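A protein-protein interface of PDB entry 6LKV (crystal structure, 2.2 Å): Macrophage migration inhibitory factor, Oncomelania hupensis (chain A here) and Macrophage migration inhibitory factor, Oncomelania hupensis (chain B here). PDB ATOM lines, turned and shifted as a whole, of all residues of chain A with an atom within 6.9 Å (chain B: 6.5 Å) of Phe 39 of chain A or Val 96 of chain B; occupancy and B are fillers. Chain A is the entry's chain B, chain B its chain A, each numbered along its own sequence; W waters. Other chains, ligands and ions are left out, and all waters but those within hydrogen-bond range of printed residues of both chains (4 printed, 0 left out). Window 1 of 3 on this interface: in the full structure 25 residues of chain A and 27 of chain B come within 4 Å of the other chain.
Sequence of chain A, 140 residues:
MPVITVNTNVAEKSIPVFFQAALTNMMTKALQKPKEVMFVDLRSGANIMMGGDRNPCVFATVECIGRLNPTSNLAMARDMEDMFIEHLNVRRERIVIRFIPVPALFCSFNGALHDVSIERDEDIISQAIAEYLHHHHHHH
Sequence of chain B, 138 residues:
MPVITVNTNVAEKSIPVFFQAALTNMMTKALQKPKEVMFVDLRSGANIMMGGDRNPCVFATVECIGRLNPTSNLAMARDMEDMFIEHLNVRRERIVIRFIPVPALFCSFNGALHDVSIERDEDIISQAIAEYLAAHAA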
ATOM      1  N   MET A   1     -19.628  -0.612 -19.621  1.00  0.00           N
ATOM      2  CA  MET A   1     -19.906   0.412 -20.649  1.00  0.00           C
ATOM      3  C   MET A   1     -20.604  -0.232 -21.867  1.00  0.00           C
ATOM      4  O   MET A   1     -20.470  -1.451 -22.086  1.00  0.00           O
ATOM      5  CB  MET A   1     -18.583   1.086 -21.028  1.00  0.00           C
ATOM      6  CG  MET A   1     -17.961   0.450 -22.232  1.00  0.00           C
ATOM      7  SD  MET A   1     -18.647   1.052 -23.811  1.00  0.00           S
ATOM      8  CE  MET A   1     -18.303  -0.385 -24.835  1.00  0.00           C
ATOM      9  N   PRO A   2     -21.407   0.531 -22.691  1.00  0.00           N
ATOM     10  CA  PRO A   2     -21.865   1.862 -22.336  1.00  0.00           C
ATOM     11  C   PRO A   2     -22.953   1.609 -21.284  1.00  0.00           C
ATOM     12  O   PRO A   2     -23.738   0.659 -21.390  1.00  0.00           O
ATOM     13  CB  PRO A   2     -22.323   2.532 -23.630  1.00  0.00           C
ATOM     14  CG  PRO A   2     -22.080   1.493 -24.696  1.00  0.00           C
ATOM     15  CD  PRO A   2     -21.919   0.160 -23.997  1.00  0.00           C
ATOM     16  N   VAL A   3     -22.871   2.370 -20.215  1.00  0.00           N
ATOM     17  CA  VAL A   3     -23.860   2.325 -19.116  1.00  0.00           C
ATOM     18  C   VAL A   3     -24.314   3.750 -18.918  1.00  0.00           C
ATOM     19  O   VAL A   3     -23.451   4.615 -18.692  1.00  0.00           O
ATOM     20  CB  VAL A   3     -23.243   1.739 -17.842  1.00  0.00           C
ATOM     21  CG1 VAL A   3     -24.254   1.707 -16.714  1.00  0.00           C
ATOM     22  CG2 VAL A   3     -22.624   0.384 -18.105  1.00  0.00           C
ATOM     23  N   ILE A   4     -25.615   3.969 -19.064  1.00  0.00           N
ATOM     24  CA  ILE A   4     -26.286   5.265 -18.770  1.00  0.00           C
ATOM     25  C   ILE A   4     -26.988   5.060 -17.434  1.00  0.00           C
ATOM     26  O   ILE A   4     -27.907   4.167 -17.351  1.00  0.00           O
ATOM     27  CB  ILE A   4     -27.295   5.636 -19.876  1.00  0.00           C
ATOM     28  CG1 ILE A   4     -26.805   5.260 -21.280  1.00  0.00           C
ATOM     29  CG2 ILE A   4     -27.716   7.086 -19.775  1.00  0.00           C
ATOM     30  CD1 ILE A   4     -25.528   5.909 -21.715  1.00  0.00           C
ATOM     31  N   THR A   5     -26.585   5.807 -16.418  1.00  0.00           N
ATOM     32  CA  THR A   5     -27.210   5.750 -15.070  1.00  0.00           C
ATOM     33  C   THR A   5     -27.999   7.045 -14.878  1.00  0.00           C
ATOM     34  O   THR A   5     -27.418   8.145 -15.024  1.00  0.00           O
ATOM     35  CB  THR A   5     -26.145   5.494 -13.992  1.00  0.00           C
ATOM     36  OG1 THR A   5     -25.378   4.350 -14.387  1.00  0.00           O
ATOM     37  CG2 THR A   5     -26.729   5.248 -12.615  1.00  0.00           C
ATOM     38  N   THR A  24     -32.111   4.142 -24.414  1.00  0.00           N
ATOM     39  CA  THR A  24     -31.261   3.093 -25.019  1.00  0.00           C
ATOM     40  C   THR A  24     -31.083   3.409 -26.508  1.00  0.00           C
ATOM     41  O   THR A  24     -29.928   3.516 -26.960  1.00  0.00           O
ATOM     42  CB  THR A  24     -31.857   1.703 -24.834  1.00  0.00           C
ATOM     43  OG1 THR A  24     -31.950   1.366 -23.453  1.00  0.00           O
ATOM     44  CG2 THR A  24     -31.069   0.625 -25.549  1.00  0.00           C
ATOM     45  N   LYS A  35     -26.228  -1.970 -29.647  1.00  0.00           N
ATOM     46  CA  LYS A  35     -27.390  -1.858 -28.733  1.00  0.00           C
ATOM     47  C   LYS A  35     -27.268  -2.933 -27.637  1.00  0.00           C
ATOM     48  O   LYS A  35     -27.633  -2.654 -26.509  1.00  0.00           O
ATOM     49  CB  LYS A  35     -28.693  -2.002 -29.529  1.00  0.00           C
ATOM     50  CG  LYS A  35     -29.950  -1.798 -28.693  1.00  0.00           C
ATOM     51  CD  LYS A  35     -31.201  -1.556 -29.510  1.00  0.00           C
ATOM     52  CE  LYS A  35     -32.460  -1.984 -28.781  1.00  0.00           C
ATOM     53  NZ  LYS A  35     -33.660  -1.296 -29.306  1.00  0.00           N
ATOM     54  N   GLU A  36     -26.734  -4.101 -27.977  1.00  0.00           N
ATOM     55  CA  GLU A  36     -26.674  -5.323 -27.143  1.00  0.00           C
ATOM     56  C   GLU A  36     -25.987  -5.028 -25.800  1.00  0.00           C
ATOM     57  O   GLU A  36     -26.333  -5.695 -24.817  1.00  0.00           O
ATOM     58  CB  GLU A  36     -25.887  -6.419 -27.870  1.00  0.00           C
ATOM     59  CG  GLU A  36     -26.653  -7.093 -29.000  1.00  0.00           C
ATOM     60  CD  GLU A  36     -26.876  -6.286 -30.276  1.00  0.00           C
ATOM     61  OE1 GLU A  36     -26.113  -5.326 -30.543  1.00  0.00           O
ATOM     62  OE2 GLU A  36     -27.836  -6.628 -31.008  1.00  0.00           O
ATOM     63  N   VAL A  37     -25.008  -4.119 -25.781  1.00  0.00           N
ATOM     64  CA  VAL A  37     -24.180  -3.832 -24.577  1.00  0.00           C
ATOM     65  C   VAL A  37     -24.565  -2.465 -24.000  1.00  0.00           C
ATOM     66  O   VAL A  37     -23.841  -1.976 -23.160  1.00  0.00           O
ATOM     67  CB  VAL A  37     -22.670  -3.939 -24.888  1.00  0.00           C
ATOM     68  CG1 VAL A  37     -22.315  -5.343 -25.337  1.00  0.00           C
ATOM     69  CG2 VAL A  37     -22.208  -2.923 -25.922  1.00  0.00           C
ATOM     70  N   MET A  38     -25.672  -1.867 -24.427  1.00  0.00           N
ATOM     71  CA  MET A  38     -26.152  -0.587 -23.849  1.00  0.00           C
ATOM     72  C   MET A  38     -26.975  -0.907 -22.599  1.00  0.00           C
ATOM     73  O   MET A  38     -28.041  -1.550 -22.695  1.00  0.00           O
ATOM     74  CB  MET A  38     -27.001   0.210 -24.845  1.00  0.00           C
ATOM     75  CG  MET A  38     -27.423   1.579 -24.343  1.00  0.00           C
ATOM     76  SD  MET A  38     -26.082   2.821 -24.297  1.00  0.00           S
ATOM     77  CE  MET A  38     -25.274   2.473 -25.860  1.00  0.00           C
ATOM     78  N   PHE A  39     -26.479  -0.484 -21.446  1.00  0.00           N
ATOM     79  CA  PHE A  39     -27.220  -0.552 -20.172  1.00  0.00           C
ATOM     80  C   PHE A  39     -27.886   0.779 -19.919  1.00  0.00           C
ATOM     81  O   PHE A  39     -27.210   1.798 -20.111  1.00  0.00           O
ATOM     82  CB  PHE A  39     -26.319  -0.846 -18.990  1.00  0.00           C
ATOM     83  CG  PHE A  39     -25.779  -2.243 -18.927  1.00  0.00           C
ATOM     84  CD1 PHE A  39     -24.652  -2.612 -19.655  1.00  0.00           C
ATOM     85  CD2 PHE A  39     -26.348  -3.158 -18.072  1.00  0.00           C
ATOM     86  CE1 PHE A  39     -24.157  -3.903 -19.568  1.00  0.00           C
ATOM     87  CE2 PHE A  39     -25.844  -4.449 -17.967  1.00  0.00           C
ATOM     88  CZ  PHE A  39     -24.732  -4.805 -18.706  1.00  0.00           C
ATOM     89  N   VAL A  40     -29.156   0.751 -19.484  1.00  0.00           N
ATOM     90  CA  VAL A  40     -29.781   1.932 -18.830  1.00  0.00           C
ATOM     91  C   VAL A  40     -30.253   1.516 -17.433  1.00  0.00           C
ATOM     92  O   VAL A  40     -31.124   0.600 -17.304  1.00  0.00           O
ATOM     93  CB  VAL A  40     -30.910   2.535 -19.674  1.00  0.00           C
ATOM     94  CG1 VAL A  40     -31.500   3.752 -18.988  1.00  0.00           C
ATOM     95  CG2 VAL A  40     -30.423   2.888 -21.062  1.00  0.00           C
ATOM     96  N   ASP A  41     -29.658   2.153 -16.438  1.00  0.00           N
ATOM     97  CA  ASP A  41     -29.916   1.901 -14.998  1.00  0.00           C
ATOM     98  C   ASP A  41     -30.690   3.101 -14.485  1.00  0.00           C
ATOM     99  O   ASP A  41     -30.079   4.157 -14.313  1.00  0.00           O
ATOM    100  CB  ASP A  41     -28.616   1.681 -14.241  1.00  0.00           C
ATOM    101  CG  ASP A  41     -28.784   1.251 -12.799  1.00  0.00           C
ATOM    102  OD1 ASP A  41     -29.948   1.175 -12.316  1.00  0.00           O
ATOM    103  OD2 ASP A  41     -27.727   0.926 -12.217  1.00  0.00           O
ATOM    104  N   CYS A 107     -12.297  -2.957 -18.506  1.00  0.00           N
ATOM    105  CA  CYS A 107     -13.741  -3.252 -18.695  1.00  0.00           C
ATOM    106  C   CYS A 107     -13.899  -4.590 -19.409  1.00  0.00           C
ATOM    107  O   CYS A 107     -13.391  -4.710 -20.577  1.00  0.00           O
ATOM    108  CB  CYS A 107     -14.455  -2.134 -19.442  1.00  0.00           C
ATOM    109  SG  CYS A 107     -16.254  -2.372 -19.494  1.00  0.00           S
ATOM    110  N   SER A 108     -14.560  -5.544 -18.752  1.00  0.00           N
ATOM    111  CA  SER A 108     -14.894  -6.875 -19.308  1.00  0.00           C
ATOM    112  C   SER A 108     -16.329  -6.902 -19.865  1.00  0.00           C
ATOM    113  O   SER A 108     -17.225  -6.247 -19.315  1.00  0.00           O
ATOM    114  CB  SER A 108     -14.659  -7.960 -18.311  1.00  0.00           C
ATOM    115  OG  SER A 108     -15.542  -7.892 -17.203  1.00  0.00           O
ATOM    116  N   PHE A 109     -16.509  -7.630 -20.960  1.00  0.00           N
ATOM    117  CA  PHE A 109     -17.818  -8.049 -21.510  1.00  0.00           C
ATOM    118  C   PHE A 109     -17.644  -9.474 -22.003  1.00  0.00           C
ATOM    119  O   PHE A 109     -16.707  -9.734 -22.786  1.00  0.00           O
ATOM    120  CB  PHE A 109     -18.323  -7.137 -22.631  1.00  0.00           C
ATOM    121  CG  PHE A 109     -19.450  -7.738 -23.427  1.00  0.00           C
ATOM    122  CD1 PHE A 109     -20.630  -8.113 -22.797  1.00  0.00           C
ATOM    123  CD2 PHE A 109     -19.318  -7.997 -24.789  1.00  0.00           C
ATOM    124  CE1 PHE A 109     -21.670  -8.697 -23.509  1.00  0.00           C
ATOM    125  CE2 PHE A 109     -20.361  -8.565 -25.516  1.00  0.00           C
ATOM    126  CZ  PHE A 109     -21.530  -8.926 -24.873  1.00  0.00           C
ATOM    127  N   ASN A 110     -18.501 -10.372 -21.518  1.00  0.00           N
ATOM    128  CA  ASN A 110     -18.638 -11.737 -22.064  1.00  0.00           C
ATOM    129  C   ASN A 110     -17.272 -12.435 -22.074  1.00  0.00           C
ATOM    130  O   ASN A 110     -16.931 -13.018 -23.096  1.00  0.00           O
ATOM    131  CB  ASN A 110     -19.226 -11.674 -23.478  1.00  0.00           C
ATOM    132  CG  ASN A 110     -19.682 -13.016 -24.006  1.00  0.00           C
ATOM    133  OD1 ASN A 110     -20.077 -13.882 -23.216  1.00  0.00           O
ATOM    134  ND2 ASN A 110     -19.620 -13.175 -25.328  1.00  0.00           N
ATOM    135  N   HIS A 114     -11.782  -5.328 -23.793  1.00  0.00           N
ATOM    136  CA  HIS A 114     -12.151  -4.631 -25.043  1.00  0.00           C
ATOM    137  C   HIS A 114     -10.879  -4.230 -25.806  1.00  0.00           C
ATOM    138  O   HIS A 114      -9.797  -4.154 -25.181  1.00  0.00           O
ATOM    139  CB  HIS A 114     -13.020  -3.414 -24.707  1.00  0.00           C
ATOM    140  CG  HIS A 114     -14.373  -3.758 -24.206  1.00  0.00           C
ATOM    141  ND1 HIS A 114     -14.593  -4.156 -22.894  1.00  0.00           N
ATOM    142  CD2 HIS A 114     -15.576  -3.737 -24.812  1.00  0.00           C
ATOM    143  CE1 HIS A 114     -15.878  -4.378 -22.718  1.00  0.00           C
ATOM    144  NE2 HIS A 114     -16.507  -4.127 -23.887  1.00  0.00           N
ATOM    145  N   ASN B   7     -24.844  -4.353  -9.795  1.00  0.00           N
ATOM    146  CA  ASN B   7     -26.114  -3.762 -10.255  1.00  0.00           C
ATOM    147  C   ASN B   7     -26.772  -4.845 -11.093  1.00  0.00           C
ATOM    148  O   ASN B   7     -26.190  -5.184 -12.117  1.00  0.00           O
ATOM    149  CB  ASN B   7     -25.924  -2.481 -11.063  1.00  0.00           C
ATOM    150  CG  ASN B   7     -25.158  -1.438 -10.294  1.00  0.00           C
ATOM    151  OD1 ASN B   7     -25.753  -0.757  -9.465  1.00  0.00           O
ATOM    152  ND2 ASN B   7     -23.874  -1.283 -10.606  1.00  0.00           N
ATOM    153  N   ILE B  48     -32.572  -1.960 -14.082  1.00  0.00           N
ATOM    154  CA  ILE B  48     -31.464  -1.929 -15.058  1.00  0.00           C
ATOM    155  C   ILE B  48     -31.852  -2.873 -16.197  1.00  0.00           C
ATOM    156  O   ILE B  48     -32.213  -4.022 -15.940  1.00  0.00           O
ATOM    157  CB  ILE B  48     -30.100  -2.266 -14.410  1.00  0.00           C
ATOM    158  CG1 ILE B  48     -28.949  -2.139 -15.427  1.00  0.00           C
ATOM    159  CG2 ILE B  48     -30.110  -3.655 -13.772  1.00  0.00           C
ATOM    160  CD1 ILE B  48     -27.571  -2.100 -14.806  1.00  0.00           C
ATOM    161  N   MET B  49     -31.828  -2.334 -17.405  1.00  0.00           N
ATOM    162  CA  MET B  49     -32.042  -3.122 -18.632  1.00  0.00           C
ATOM    163  C   MET B  49     -30.746  -3.066 -19.455  1.00  0.00           C
ATOM    164  O   MET B  49     -29.926  -2.129 -19.296  1.00  0.00           O
ATOM    165  CB  MET B  49     -33.249  -2.607 -19.428  1.00  0.00           C
ATOM    166  CG  MET B  49     -33.113  -1.204 -19.959  1.00  0.00           C
ATOM    167  SD  MET B  49     -34.317  -0.857 -21.332  1.00  0.00           S
ATOM    168  CE  MET B  49     -35.850  -1.243 -20.468  1.00  0.00           C
ATOM    169  N   MET B  50     -30.582  -4.054 -20.320  1.00  0.00           N
ATOM    170  CA  MET B  50     -29.410  -4.150 -21.216  1.00  0.00           C
ATOM    171  C   MET B  50     -29.898  -4.535 -22.608  1.00  0.00           C
ATOM    172  O   MET B  50     -30.691  -5.481 -22.705  1.00  0.00           O
ATOM    173  CB  MET B  50     -28.489  -5.232 -20.647  1.00  0.00           C
ATOM    174  CG  MET B  50     -27.197  -5.422 -21.402  1.00  0.00           C
ATOM    175  SD  MET B  50     -26.378  -6.927 -20.829  1.00  0.00           S
ATOM    176  CE  MET B  50     -24.896  -6.757 -21.825  1.00  0.00           C
ATOM    177  N   GLY B  51     -29.439  -3.834 -23.632  1.00  0.00           N
ATOM    178  CA  GLY B  51     -29.886  -4.079 -25.019  1.00  0.00           C
ATOM    179  C   GLY B  51     -31.384  -3.822 -25.207  1.00  0.00           C
ATOM    180  O   GLY B  51     -31.957  -4.420 -26.105  1.00  0.00           O
ATOM    181  N   CYS B  57     -29.394  -9.419 -16.206  1.00  0.00           N
ATOM    182  CA  CYS B  57     -28.096  -8.785 -16.558  1.00  0.00           C
ATOM    183  C   CYS B  57     -27.372  -8.302 -15.293  1.00  0.00           C
ATOM    184  O   CYS B  57     -27.999  -8.233 -14.208  1.00  0.00           O
ATOM    185  CB  CYS B  57     -28.326  -7.656 -17.541  1.00  0.00           C
ATOM    186  SG  CYS B  57     -29.199  -6.209 -16.877  1.00  0.00           S
ATOM    187  N   VAL B  58     -26.076  -8.019 -15.426  1.00  0.00           N
ATOM    188  CA  VAL B  58     -25.216  -7.474 -14.336  1.00  0.00           C
ATOM    189  C   VAL B  58     -24.316  -6.398 -14.936  1.00  0.00           C
ATOM    190  O   VAL B  58     -23.596  -6.715 -15.904  1.00  0.00           O
ATOM    191  CB  VAL B  58     -24.359  -8.558 -13.662  1.00  0.00           C
ATOM    192  CG1 VAL B  58     -23.450  -7.950 -12.608  1.00  0.00           C
ATOM    193  CG2 VAL B  58     -25.204  -9.653 -13.058  1.00  0.00           C
ATOM    194  N   PHE B  59     -24.334  -5.198 -14.366  1.00  0.00           N
ATOM    195  CA  PHE B  59     -23.218  -4.233 -14.487  1.00  0.00           C
ATOM    196  C   PHE B  59     -22.566  -4.123 -13.106  1.00  0.00           C
ATOM    197  O   PHE B  59     -23.244  -3.754 -12.125  1.00  0.00           O
ATOM    198  CB  PHE B  59     -23.658  -2.882 -15.025  1.00  0.00           C
ATOM    199  CG  PHE B  59     -22.539  -1.875 -15.018  1.00  0.00           C
ATOM    200  CD1 PHE B  59     -21.339  -2.163 -15.650  1.00  0.00           C
ATOM    201  CD2 PHE B  59     -22.662  -0.677 -14.341  1.00  0.00           C
ATOM    202  CE1 PHE B  59     -20.285  -1.259 -15.629  1.00  0.00           C
ATOM    203  CE2 PHE B  59     -21.609   0.227 -14.310  1.00  0.00           C
ATOM    204  CZ  PHE B  59     -20.428  -0.052 -14.985  1.00  0.00           C
ATOM    205  N   ALA B  60     -21.307  -4.524 -13.006  1.00  0.00           N
ATOM    206  CA  ALA B  60     -20.555  -4.536 -11.734  1.00  0.00           C
ATOM    207  C   ALA B  60     -19.330  -3.630 -11.843  1.00  0.00           C
ATOM    208  O   ALA B  60     -18.786  -3.487 -12.947  1.00  0.00           O
ATOM    209  CB  ALA B  60     -20.195  -5.948 -11.346  1.00  0.00           C
ATOM    210  N   THR B  61     -18.927  -3.035 -10.730  1.00  0.00           N
ATOM    211  CA  THR B  61     -17.726  -2.185 -10.643  1.00  0.00           C
ATOM    212  C   THR B  61     -16.822  -2.705  -9.530  1.00  0.00           C
ATOM    213  O   THR B  61     -17.337  -3.164  -8.478  1.00  0.00           O
ATOM    214  CB  THR B  61     -18.086  -0.710 -10.499  1.00  0.00           C
ATOM    215  OG1 THR B  61     -18.811  -0.536  -9.293  1.00  0.00           O
ATOM    216  CG2 THR B  61     -18.878  -0.203 -11.693  1.00  0.00           C
ATOM    217  N   GLU B  81     -17.742 -13.226 -13.200  1.00  0.00           N
ATOM    218  CA  GLU B  81     -18.707 -13.774 -14.187  1.00  0.00           C
ATOM    219  C   GLU B  81     -19.194 -15.146 -13.738  1.00  0.00           C
ATOM    220  O   GLU B  81     -20.435 -15.368 -13.648  1.00  0.00           O
ATOM    221  CB  GLU B  81     -18.068 -13.838 -15.565  1.00  0.00           C
ATOM    222  CG  GLU B  81     -18.076 -12.536 -16.299  1.00  0.00           C
ATOM    223  CD  GLU B  81     -17.320 -12.579 -17.613  1.00  0.00           C
ATOM    224  OE1 GLU B  81     -16.683 -13.636 -17.842  1.00  0.00           O
ATOM    225  OE2 GLU B  81     -17.324 -11.554 -18.380  1.00  0.00           O
ATOM    226  N   PHE B  84     -21.553 -14.918 -10.955  1.00  0.00           N
ATOM    227  CA  PHE B  84     -22.851 -14.348 -11.397  1.00  0.00           C
ATOM    228  C   PHE B  84     -23.671 -15.427 -12.135  1.00  0.00           C
ATOM    229  O   PHE B  84     -24.890 -15.554 -11.906  1.00  0.00           O
ATOM    230  CB  PHE B  84     -22.634 -13.086 -12.227  1.00  0.00           C
ATOM    231  CG  PHE B  84     -21.920 -11.940 -11.548  1.00  0.00           C
ATOM    232  CD1 PHE B  84     -21.948 -11.791 -10.177  1.00  0.00           C
ATOM    233  CD2 PHE B  84     -21.280 -10.957 -12.294  1.00  0.00           C
ATOM    234  CE1 PHE B  84     -21.299 -10.724  -9.563  1.00  0.00           C
ATOM    235  CE2 PHE B  84     -20.608  -9.901 -11.686  1.00  0.00           C
ATOM    236  CZ  PHE B  84     -20.625  -9.785 -10.322  1.00  0.00           C
ATOM    237  N   ARG B  92     -23.166 -15.126 -19.419  1.00  0.00           N
ATOM    238  CA  ARG B  92     -21.893 -14.362 -19.526  1.00  0.00           C
ATOM    239  C   ARG B  92     -22.086 -13.157 -20.450  1.00  0.00           C
ATOM    240  O   ARG B  92     -21.505 -12.100 -20.181  1.00  0.00           O
ATOM    241  CB  ARG B  92     -20.735 -15.237 -20.017  1.00  0.00           C
ATOM    242  CG  ARG B  92     -19.374 -14.710 -19.570  1.00  0.00           C
ATOM    243  CD  ARG B  92     -18.232 -15.562 -20.113  1.00  0.00           C
ATOM    244  NE  ARG B  92     -18.219 -16.879 -19.483  1.00  0.00           N
ATOM    245  CZ  ARG B  92     -17.719 -17.161 -18.284  1.00  0.00           C
ATOM    246  NH1 ARG B  92     -17.152 -16.232 -17.532  1.00  0.00           N
ATOM    247  NH2 ARG B  92     -17.783 -18.381 -17.809  1.00  0.00           N
ATOM    248  N   ARG B  94     -24.482 -11.256 -20.730  1.00  0.00           N
ATOM    249  CA  ARG B  94     -25.302 -10.208 -20.069  1.00  0.00           C
ATOM    250  C   ARG B  94     -24.527  -9.597 -18.876  1.00  0.00           C
ATOM    251  O   ARG B  94     -25.182  -9.038 -17.972  1.00  0.00           O
ATOM    252  CB  ARG B  94     -26.624 -10.841 -19.651  1.00  0.00           C
ATOM    253  CG  ARG B  94     -27.448 -11.337 -20.830  1.00  0.00           C
ATOM    254  CD  ARG B  94     -28.161 -10.241 -21.585  1.00  0.00           C
ATOM    255  NE  ARG B  94     -29.185  -9.620 -20.759  1.00  0.00           N
ATOM    256  CZ  ARG B  94     -29.934  -8.587 -21.151  1.00  0.00           C
ATOM    257  NH1 ARG B  94     -29.744  -8.051 -22.343  1.00  0.00           N
ATOM    258  NH2 ARG B  94     -30.848  -8.077 -20.336  1.00  0.00           N
ATOM    259  N   ILE B  95     -23.195  -9.716 -18.876  1.00  0.00           N
ATOM    260  CA  ILE B  95     -22.313  -9.229 -17.769  1.00  0.00           C
ATOM    261  C   ILE B  95     -21.235  -8.287 -18.315  1.00  0.00           C
ATOM    262  O   ILE B  95     -20.486  -8.649 -19.244  1.00  0.00           O
ATOM    263  CB  ILE B  95     -21.686 -10.395 -17.007  1.00  0.00           C
ATOM    264  CG1 ILE B  95     -22.750 -11.354 -16.472  1.00  0.00           C
ATOM    265  CG2 ILE B  95     -20.801  -9.867 -15.884  1.00  0.00           C
ATOM    266  CD1 ILE B  95     -22.179 -12.652 -15.954  1.00  0.00           C
ATOM    267  N   VAL B  96     -21.187  -7.094 -17.757  1.00  0.00           N
ATOM    268  CA  VAL B  96     -20.130  -6.074 -17.975  1.00  0.00           C
ATOM    269  C   VAL B  96     -19.590  -5.694 -16.592  1.00  0.00           C
ATOM    270  O   VAL B  96     -20.414  -5.503 -15.667  1.00  0.00           O
ATOM    271  CB  VAL B  96     -20.648  -4.856 -18.748  1.00  0.00           C
ATOM    272  CG1 VAL B  96     -19.618  -3.727 -18.742  1.00  0.00           C
ATOM    273  CG2 VAL B  96     -21.014  -5.242 -20.184  1.00  0.00           C
ATOM    274  N   ILE B  97     -18.268  -5.689 -16.451  1.00  0.00           N
ATOM    275  CA  ILE B  97     -17.570  -5.294 -15.204  1.00  0.00           C
ATOM    276  C   ILE B  97     -16.604  -4.169 -15.552  1.00  0.00           C
ATOM    277  O   ILE B  97     -15.843  -4.317 -16.503  1.00  0.00           O
ATOM    278  CB  ILE B  97     -16.860  -6.492 -14.545  1.00  0.00           C
ATOM    279  CG1 ILE B  97     -17.800  -7.673 -14.387  1.00  0.00           C
ATOM    280  CG2 ILE B  97     -16.227  -6.065 -13.236  1.00  0.00           C
ATOM    281  CD1 ILE B  97     -17.132  -8.974 -14.000  1.00  0.00           C
ATOM    282  N   ARG B  98     -16.641  -3.090 -14.789  1.00  0.00           N
ATOM    283  CA  ARG B  98     -15.689  -1.977 -14.893  1.00  0.00           C
ATOM    284  C   ARG B  98     -14.743  -2.015 -13.696  1.00  0.00           C
ATOM    285  O   ARG B  98     -15.234  -2.073 -12.543  1.00  0.00           O
ATOM    286  CB  ARG B  98     -16.419  -0.651 -14.965  1.00  0.00           C
ATOM    287  CG  ARG B  98     -15.470   0.503 -15.194  1.00  0.00           C
ATOM    288  CD  ARG B  98     -16.187   1.817 -15.164  1.00  0.00           C
ATOM    289  NE  ARG B  98     -15.203   2.842 -14.895  1.00  0.00           N
ATOM    290  CZ  ARG B  98     -15.454   3.969 -14.275  1.00  0.00           C
ATOM    291  NH1 ARG B  98     -16.682   4.262 -13.878  1.00  0.00           N
ATOM    292  NH2 ARG B  98     -14.465   4.800 -14.034  1.00  0.00           N
HETATM  293  O   HOH W   1     -27.712  -8.049 -24.629  1.00  0.00           O
HETATM  294  O   HOH W   2     -30.809  -1.131 -22.422  1.00  0.00           O
HETATM  295  O   HOH W   3     -28.507   0.061  -9.686  1.00  0.00           O
HETATM  296  O   HOH W   4     -17.810  -9.151 -18.049  1.00  0.00           O
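The backbone NH (N) of Ile 4 of chain A is in hydrogen-bond range of the backbone carbonyl oxygen (O) of Phe 39 of chain A (2.9 Å).
Water W2 lies within hydrogen-bond range of O of Met 38 of chain A (2.8 Å), OG1 of Thr 24 of chain A (2.9 Å), N of Gly 51 of chain B (3.3 Å) and O of Met 49 of chain B (3.4 Å).
O of Ile 95 of chain B sits at hydrogen-bond distance from N of Asn 110 of chain A, 3.5 Å away. The backbone carbonyl oxygen (O) of Met 49 of chain B is in hydrogen-bond range of the backbone NH (N) of Val 40 of chain A, 3.0 Å away. The backbone NH (N) of Gly 51 of chain B is in hydrogen-bond range of the backbone carbonyl oxygen (O) of Met 38 of chain A, 2.8 Å away. N of Ser 108 of chain A is in hydrogen-bond range of O of Ile 97 of chain B (2.9 Å). O of Ile 97 of chain B sits close to SG of Cys 107 of chain A (3.6 Å).
Among the printed residues, merely in contact across the chains: Lys 35 of chain A with Gly 51 of chain B (3.1 Å), Ser 108 of chain A with Val 96 of chain B (3.2 Å), Met 1 of chain A with Val 96 of chain B (3.2 Å), Phe 39 of chain A with Met 49 of chain B (3.3 Å), Met 38 of chain A with Met 50 of chain B (3.3 Å), Val 40 of chain A with Ile 48 of chain B (3.4 Å), Phe 39 of chain A with Met 50 of chain B (3.4 Å), Asn 110 of chain A with Arg 92 of chain B (3.4 Å), Phe 39 of chain A with Val 96 of chain B (3.5 Å), Glu 36 of chain A with Met 50 of chain B (3.5 Å), Phe 109 of chain A with Ile 95 of chain B (3.6 Å), Asn 110 of chain A with Glu 81 of chain B (3.6 Å), Phe 39 of chain A with Val 58 of chain B (3.6 Å), Phe 39 of chain A with Ile 48 of chain B (3.6 Å), Cys 107 of chain A with Val 96 of chain B (3.7 Å), Val 3 of chain A with Phe 59 of chain B (3.7 Å), Asp 41 of chain A with Asn 7 of chain B (3.8 Å), Glu 36 of chain A with Gly 51 of chain B (3.8 Å), Thr 24 of chain A with Met 49 of chain B (3.9 Å), Phe 109 of chain A with Val 96 of chain B (3.9 Å), Met 38 of chain A with Met 49 of chain B (3.9 Å), Phe 39 of chain A with Cys 57 of chain B (3.9 Å), Asp 41 of chain A with Ile 48 of chain B (3.96 Å) and Phe 39 of chain A with Phe 59 of chain B (3.98 Å).
Hydrophobic or aromatic side chains of chain B that line the printed part of chain A: Ile 48, Met 49, Met 50, Phe 59, Val 96 and Ile 97. Printed residues of chain A that touch a printed residue of chain B: Met 1, Val 3, Thr 24, Lys 35, Glu 36, Met 38, Phe 39, Val 40, Asp 41, Cys 107, Ser 108, Phe 109 and Asn 110. Among the printed residues, no Asp or Glu carboxylate lies within 4 Å of a Lys or Arg side-chain nitrogen of the other chain.
Printed residues of chain B within 4 Å of Met 38 of chain A: Met 49 (3.9 Å), Met 50 (3.3 Å) and Gly 51 (2.8 Å). Phe 39 of chain A touches just these residues of chain B: Ile 48, Met 49, Met 50, Cys 57, Val 58, Phe 59 and Val 96. Of the printed residues of chain A, Glu 81 of chain B touches Asn 110. Val 96 of chain B touches five residues of chain A. The nearest residue of chain B that does not touch Phe 39 of chain A is Arg 94 of chain B (4.3 Å). The nearest printed residue of chain A that does not touch Val 96 of chain B is Val 3 of chain A (5.1 Å). The nearest printed residue of chain B that does not touch Asn 110 of chain A is Val 96 of chain B (5.7 Å).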
